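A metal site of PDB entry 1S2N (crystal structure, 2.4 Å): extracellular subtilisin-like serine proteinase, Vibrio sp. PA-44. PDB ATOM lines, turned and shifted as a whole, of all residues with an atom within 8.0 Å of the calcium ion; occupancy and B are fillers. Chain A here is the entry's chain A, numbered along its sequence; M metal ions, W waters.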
ATOM      1  N   GLN A   1       0.791 -20.874   0.510  1.00  0.00           N
ATOM      2  CA  GLN A   1       0.620 -19.781   1.513  1.00  0.00           C
ATOM      3  C   GLN A   1       1.024 -18.430   0.901  1.00  0.00           C
ATOM      4  O   GLN A   1       2.118 -18.313   0.361  1.00  0.00           O
ATOM      5  CB  GLN A   1       1.458 -20.070   2.770  1.00  0.00           C
ATOM      6  CG  GLN A   1       0.636 -20.429   4.017  1.00  0.00           C
ATOM      7  CD  GLN A   1       1.471 -20.443   5.289  1.00  0.00           C
ATOM      8  OE1 GLN A   1       1.181 -19.715   6.246  1.00  0.00           O
ATOM      9  NE2 GLN A   1       2.518 -21.288   5.307  1.00  0.00           N
ATOM     10  N   ALA A   4       4.351 -16.574   3.025  1.00  0.00           N
ATOM     11  CA  ALA A   4       5.156 -17.585   3.716  1.00  0.00           C
ATOM     12  C   ALA A   4       6.495 -17.008   4.180  1.00  0.00           C
ATOM     13  O   ALA A   4       7.125 -16.236   3.462  1.00  0.00           O
ATOM     14  CB  ALA A   4       5.405 -18.771   2.806  1.00  0.00           C
ATOM     15  N   ILE A   5       6.911 -17.382   5.384  1.00  0.00           N
ATOM     16  CA  ILE A   5       8.272 -17.096   5.854  1.00  0.00           C
ATOM     17  C   ILE A   5       9.278 -17.871   5.012  1.00  0.00           C
ATOM     18  O   ILE A   5       8.945 -18.903   4.415  1.00  0.00           O
ATOM     19  CB  ILE A   5       8.432 -17.410   7.377  1.00  0.00           C
ATOM     20  CG1 ILE A   5       8.158 -18.887   7.680  1.00  0.00           C
ATOM     21  CG2 ILE A   5       7.529 -16.495   8.200  1.00  0.00           C
ATOM     22  CD1 ILE A   5       8.514 -19.300   9.104  1.00  0.00           C
ATOM     23  N   TRP A   6      10.519 -17.398   4.983  1.00  0.00           N
ATOM     24  CA  TRP A   6      11.462 -17.808   3.951  1.00  0.00           C
ATOM     25  C   TRP A   6      11.797 -19.300   3.904  1.00  0.00           C
ATOM     26  O   TRP A   6      11.991 -19.852   2.823  1.00  0.00           O
ATOM     27  CB  TRP A   6      12.754 -16.980   4.048  1.00  0.00           C
ATOM     28  CG  TRP A   6      13.809 -17.531   4.949  1.00  0.00           C
ATOM     29  CD1 TRP A   6      14.076 -17.142   6.227  1.00  0.00           C
ATOM     30  CD2 TRP A   6      14.789 -18.529   4.621  1.00  0.00           C
ATOM     31  NE1 TRP A   6      15.150 -17.853   6.723  1.00  0.00           N
ATOM     32  CE2 TRP A   6      15.606 -18.706   5.760  1.00  0.00           C
ATOM     33  CE3 TRP A   6      15.061 -19.302   3.483  1.00  0.00           C
ATOM     34  CZ2 TRP A   6      16.667 -19.611   5.783  1.00  0.00           C
ATOM     35  CZ3 TRP A   6      16.114 -20.213   3.520  1.00  0.00           C
ATOM     36  CH2 TRP A   6      16.898 -20.355   4.660  1.00  0.00           C
ATOM     37  N   GLY A   7      11.876 -19.946   5.069  1.00  0.00           N
ATOM     38  CA  GLY A   7      12.314 -21.324   5.147  1.00  0.00           C
ATOM     39  C   GLY A   7      11.343 -22.325   4.551  1.00  0.00           C
ATOM     40  O   GLY A   7      11.732 -23.264   3.872  1.00  0.00           O
ATOM     41  N   LEU A   8      10.065 -22.127   4.843  1.00  0.00           N
ATOM     42  CA  LEU A   8       9.003 -22.916   4.229  1.00  0.00           C
ATOM     43  C   LEU A   8       8.972 -22.612   2.739  1.00  0.00           C
ATOM     44  O   LEU A   8       8.855 -23.509   1.901  1.00  0.00           O
ATOM     45  CB  LEU A   8       7.642 -22.569   4.831  1.00  0.00           C
ATOM     46  CG  LEU A   8       7.434 -22.772   6.328  1.00  0.00           C
ATOM     47  CD1 LEU A   8       6.018 -22.359   6.707  1.00  0.00           C
ATOM     48  CD2 LEU A   8       7.698 -24.222   6.727  1.00  0.00           C
ATOM     49  N   ASP A   9       9.081 -21.315   2.424  1.00  0.00           N
ATOM     50  CA  ASP A   9       9.095 -20.828   1.056  1.00  0.00           C
ATOM     51  C   ASP A   9      10.177 -21.516   0.212  1.00  0.00           C
ATOM     52  O   ASP A   9       9.963 -21.791  -0.960  1.00  0.00           O
ATOM     53  CB  ASP A   9       9.321 -19.315   1.060  1.00  0.00           C
ATOM     54  CG  ASP A   9       9.061 -18.677  -0.273  1.00  0.00           C
ATOM     55  OD1 ASP A   9       9.174 -17.434  -0.336  1.00  0.00           O
ATOM     56  OD2 ASP A   9       8.723 -19.305  -1.302  1.00  0.00           O
ATOM     57  N   ARG A  10      11.324 -21.806   0.823  1.00  0.00           N
ATOM     58  CA  ARG A  10      12.471 -22.319   0.099  1.00  0.00           C
ATOM     59  C   ARG A  10      12.358 -23.801  -0.257  1.00  0.00           C
ATOM     60  O   ARG A  10      12.799 -24.218  -1.321  1.00  0.00           O
ATOM     61  CB  ARG A  10      13.744 -22.087   0.917  1.00  0.00           C
ATOM     62  CG  ARG A  10      15.038 -22.391   0.175  1.00  0.00           C
ATOM     63  CD  ARG A  10      15.297 -21.476  -1.008  1.00  0.00           C
ATOM     64  NE  ARG A  10      16.333 -22.004  -1.881  1.00  0.00           N
ATOM     65  CZ  ARG A  10      16.135 -22.884  -2.845  1.00  0.00           C
ATOM     66  NH1 ARG A  10      17.174 -23.297  -3.573  1.00  0.00           N
ATOM     67  NH2 ARG A  10      14.920 -23.352  -3.126  1.00  0.00           N
ATOM     68  N   ILE A  11      11.781 -24.596   0.647  1.00  0.00           N
ATOM     69  CA  ILE A  11      11.815 -26.053   0.514  1.00  0.00           C
ATOM     70  C   ILE A  11      10.791 -26.629  -0.485  1.00  0.00           C
ATOM     71  O   ILE A  11      10.853 -27.822  -0.770  1.00  0.00           O
ATOM     72  CB  ILE A  11      11.667 -26.744   1.895  1.00  0.00           C
ATOM     73  CG1 ILE A  11      10.355 -26.348   2.582  1.00  0.00           C
ATOM     74  CG2 ILE A  11      12.847 -26.393   2.782  1.00  0.00           C
ATOM     75  CD1 ILE A  11       9.997 -27.210   3.770  1.00  0.00           C
ATOM     76  N   ASP A  12       9.894 -25.798  -1.009  1.00  0.00           N
ATOM     77  CA  ASP A  12       8.913 -26.261  -1.999  1.00  0.00           C
ATOM     78  C   ASP A  12       9.306 -25.938  -3.448  1.00  0.00           C
ATOM     79  O   ASP A  12       8.517 -26.153  -4.372  1.00  0.00           O
ATOM     80  CB  ASP A  12       7.518 -25.676  -1.693  1.00  0.00           C
ATOM     81  CG  ASP A  12       7.339 -24.257  -2.200  1.00  0.00           C
ATOM     82  OD1 ASP A  12       6.207 -23.871  -2.528  1.00  0.00           O
ATOM     83  OD2 ASP A  12       8.283 -23.445  -2.311  1.00  0.00           O
ATOM     84  N   GLN A  13      10.525 -25.420  -3.630  1.00  0.00           N
ATOM     85  CA  GLN A  13      11.043 -25.068  -4.957  1.00  0.00           C
ATOM     86  C   GLN A  13      12.533 -25.425  -5.113  1.00  0.00           C
ATOM     87  O   GLN A  13      13.239 -25.651  -4.141  1.00  0.00           O
ATOM     88  CB  GLN A  13      10.810 -23.583  -5.252  1.00  0.00           C
ATOM     89  CG  GLN A  13      11.320 -22.601  -4.184  1.00  0.00           C
ATOM     90  CD  GLN A  13      10.885 -21.158  -4.448  1.00  0.00           C
ATOM     91  OE1 GLN A  13       9.799 -20.752  -4.017  1.00  0.00           O
ATOM     92  NE2 GLN A  13      11.721 -20.396  -5.129  1.00  0.00           N
ATOM     93  N   ARG A  14      12.981 -25.441  -6.364  1.00  0.00           N
ATOM     94  CA  ARG A  14      14.346 -25.808  -6.696  1.00  0.00           C
ATOM     95  C   ARG A  14      15.283 -24.613  -6.610  1.00  0.00           C
ATOM     96  O   ARG A  14      16.362 -24.736  -6.049  1.00  0.00           O
ATOM     97  CB  ARG A  14      14.430 -26.407  -8.106  1.00  0.00           C
ATOM     98  CG  ARG A  14      13.713 -27.743  -8.264  1.00  0.00           C
ATOM     99  CD  ARG A  14      14.212 -28.817  -7.306  1.00  0.00           C
ATOM    100  NE  ARG A  14      13.541 -30.097  -7.490  1.00  0.00           N
ATOM    101  CZ  ARG A  14      13.731 -31.158  -6.698  1.00  0.00           C
ATOM    102  NH1 ARG A  14      14.592 -31.101  -5.703  1.00  0.00           N
ATOM    103  NH2 ARG A  14      13.070 -32.293  -6.932  1.00  0.00           N
ATOM    104  N   ASN A  15      14.884 -23.485  -7.177  1.00  0.00           N
ATOM    105  CA  ASN A  15      15.767 -22.333  -7.311  1.00  0.00           C
ATOM    106  C   ASN A  15      15.227 -21.059  -6.676  1.00  0.00           C
ATOM    107  O   ASN A  15      14.017 -20.876  -6.527  1.00  0.00           O
ATOM    108  CB  ASN A  15      16.056 -22.033  -8.788  1.00  0.00           C
ATOM    109  CG  ASN A  15      16.746 -23.188  -9.493  1.00  0.00           C
ATOM    110  OD1 ASN A  15      17.830 -23.615  -9.090  1.00  0.00           O
ATOM    111  ND2 ASN A  15      16.119 -23.706 -10.544  1.00  0.00           N
ATOM    112  N   PRO A  17      14.647 -17.102  -7.425  1.00  0.00           N
ATOM    113  CA  PRO A  17      14.200 -16.382  -6.225  1.00  0.00           C
ATOM    114  C   PRO A  17      12.989 -17.008  -5.539  1.00  0.00           C
ATOM    115  O   PRO A  17      12.209 -17.753  -6.135  1.00  0.00           O
ATOM    116  CB  PRO A  17      13.822 -15.012  -6.773  1.00  0.00           C
ATOM    117  CG  PRO A  17      13.404 -15.247  -8.207  1.00  0.00           C
ATOM    118  CD  PRO A  17      14.051 -16.545  -8.650  1.00  0.00           C
ATOM    119  N   LEU A  18      12.844 -16.650  -4.254  1.00  0.00           N
ATOM    120  CA  LEU A  18      11.689 -17.032  -3.452  1.00  0.00           C
ATOM    121  C   LEU A  18      10.405 -16.434  -4.063  1.00  0.00           C
ATOM    122  O   LEU A  18      10.445 -15.387  -4.717  1.00  0.00           O
ATOM    123  CB  LEU A  18      11.886 -16.540  -2.016  1.00  0.00           C
ATOM    124  CG  LEU A  18      13.112 -17.062  -1.247  1.00  0.00           C
ATOM    125  CD1 LEU A  18      13.404 -16.208  -0.028  1.00  0.00           C
ATOM    126  CD2 LEU A  18      12.935 -18.531  -0.833  1.00  0.00           C
ATOM    127  N   ASP A  19       9.268 -17.105  -3.860  1.00  0.00           N
ATOM    128  CA  ASP A  19       7.994 -16.650  -4.431  1.00  0.00           C
ATOM    129  C   ASP A  19       6.915 -16.366  -3.383  1.00  0.00           C
ATOM    130  O   ASP A  19       5.746 -16.183  -3.726  1.00  0.00           O
ATOM    131  CB  ASP A  19       7.492 -17.635  -5.504  1.00  0.00           C
ATOM    132  CG  ASP A  19       6.970 -18.950  -4.926  1.00  0.00           C
ATOM    133  OD1 ASP A  19       6.394 -19.735  -5.694  1.00  0.00           O
ATOM    134  OD2 ASP A  19       7.098 -19.300  -3.736  1.00  0.00           O
ATOM    135  N   ARG A  20       7.311 -16.303  -2.105  1.00  0.00           N
ATOM    136  CA  ARG A  20       6.404 -16.035  -0.991  1.00  0.00           C
ATOM    137  C   ARG A  20       5.272 -17.068  -0.818  1.00  0.00           C
ATOM    138  O   ARG A  20       4.248 -16.766  -0.209  1.00  0.00           O
ATOM    139  CB  ARG A  20       5.826 -14.612  -1.124  1.00  0.00           C
ATOM    140  CG  ARG A  20       6.867 -13.501  -1.177  1.00  0.00           C
ATOM    141  CD  ARG A  20       7.488 -13.170   0.189  1.00  0.00           C
ATOM    142  N   ASN A  21       5.470 -18.267  -1.349  1.00  0.00           N
ATOM    143  CA  ASN A  21       4.505 -19.354  -1.252  1.00  0.00           C
ATOM    144  C   ASN A  21       5.105 -20.620  -0.645  1.00  0.00           C
ATOM    145  O   ASN A  21       6.229 -21.016  -0.980  1.00  0.00           O
ATOM    146  CB  ASN A  21       3.937 -19.719  -2.629  1.00  0.00           C
ATOM    147  CG  ASN A  21       3.078 -18.605  -3.239  1.00  0.00           C
ATOM    148  OD1 ASN A  21       2.109 -18.151  -2.632  1.00  0.00           O
ATOM    149  ND2 ASN A  21       3.443 -18.181  -4.438  1.00  0.00           N
ATOM    150  N   TYR A  22       4.357 -21.256   0.251  1.00  0.00           N
ATOM    151  CA  TYR A  22       4.665 -22.604   0.668  1.00  0.00           C
ATOM    152  C   TYR A  22       3.536 -23.532   0.192  1.00  0.00           C
ATOM    153  O   TYR A  22       2.423 -23.500   0.734  1.00  0.00           O
ATOM    154  CB  TYR A  22       4.854 -22.713   2.188  1.00  0.00           C
ATOM    155  CG  TYR A  22       5.022 -24.141   2.642  1.00  0.00           C
ATOM    156  CD1 TYR A  22       6.008 -24.947   2.080  1.00  0.00           C
ATOM    157  CD2 TYR A  22       4.177 -24.701   3.592  1.00  0.00           C
ATOM    158  CE1 TYR A  22       6.149 -26.270   2.453  1.00  0.00           C
ATOM    159  CE2 TYR A  22       4.319 -26.035   3.973  1.00  0.00           C
ATOM    160  CZ  TYR A  22       5.313 -26.812   3.401  1.00  0.00           C
ATOM    161  OH  TYR A  22       5.482 -28.114   3.784  1.00  0.00           O
ATOM    162  N   ASN A  23       3.845 -24.336  -0.822  1.00  0.00           N
ATOM    163  CA  ASN A  23       2.907 -25.295  -1.394  1.00  0.00           C
ATOM    164  C   ASN A  23       3.073 -26.658  -0.744  1.00  0.00           C
ATOM    165  O   ASN A  23       4.187 -27.092  -0.450  1.00  0.00           O
ATOM    166  CB  ASN A  23       3.128 -25.425  -2.909  1.00  0.00           C
ATOM    167  CG  ASN A  23       2.755 -24.155  -3.683  1.00  0.00           C
ATOM    168  OD1 ASN A  23       3.605 -23.468  -4.224  1.00  0.00           O
ATOM    169  ND2 ASN A  23       1.457 -23.859  -3.743  1.00  0.00           N
ATOM    170  N   LEU A 272       8.386 -31.714  -1.802  1.00  0.00           N
ATOM    171  CA  LEU A 272       7.382 -32.240  -2.722  1.00  0.00           C
ATOM    172  C   LEU A 272       7.895 -33.493  -3.396  1.00  0.00           C
ATOM    173  O   LEU A 272       9.092 -33.759  -3.380  1.00  0.00           O
ATOM    174  CB  LEU A 272       7.012 -31.171  -3.773  1.00  0.00           C
ATOM    175  CG  LEU A 272       6.132 -30.031  -3.244  1.00  0.00           C
ATOM    176  CD1 LEU A 272       6.956 -28.985  -2.574  1.00  0.00           C
ATOM    177  CD2 LEU A 272       5.333 -29.403  -4.360  1.00  0.00           C
HETATM  178 CA    CA M   1       7.968 -21.172  -2.564  1.00  0.00          CA
HETATM  179  O   HOH W   1       6.569 -22.019  -4.509  1.00  0.00           O
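The side-chain carboxylate of Asp 12 is in hydrogen-bond range of the backbone NH of Asn 23.
The side-chain amide oxygen (OD1) of Asn 21 sits close to the backbone carbonyl oxygen (O) of Gln 1 (3.0 Å).
The backbone carbonyl oxygen (O) of Gln 13 lies within hydrogen-bond range of the guanidinium group (NH2) of Arg 10 (3.0 Å).
The backbone carbonyl oxygen of Pro 17 lies within hydrogen-bond range of the side-chain amide nitrogen of Gln 13 (2.9 Å).
The side-chain amide nitrogen (NE2) of Gln 13 lies within hydrogen-bond range of the backbone carbonyl oxygen (O) of Asn 15 (2.7 Å).
The side-chain carboxylate (OD1) of Asp 9 lies within hydrogen-bond range of the backbone NH (N) of Arg 20.
Five residues have an atom within 4 Å of the calcium ion: Asp 9, Asp 12, Gln 13, Asp 19 and Asn 21.
The nearest printed residue that does not touch the calcium ion is Tyr 22 (4.6 Å).
The calcium ion is bound by the side-chain carboxylate of Asp 12 (2.3 Å), the backbone carbonyl oxygen of Asn 21 (2.4 Å), the side-chain carboxylate of Asp 19 (2.4 Å), the side-chain amide oxygen of Gln 13 (2.4 Å), the side-chain carboxylate of Asp 9 (2.4 Å), water W1 (2.5 Å) and the backbone carbonyl oxygen of Asp 9 (2.6 Å).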
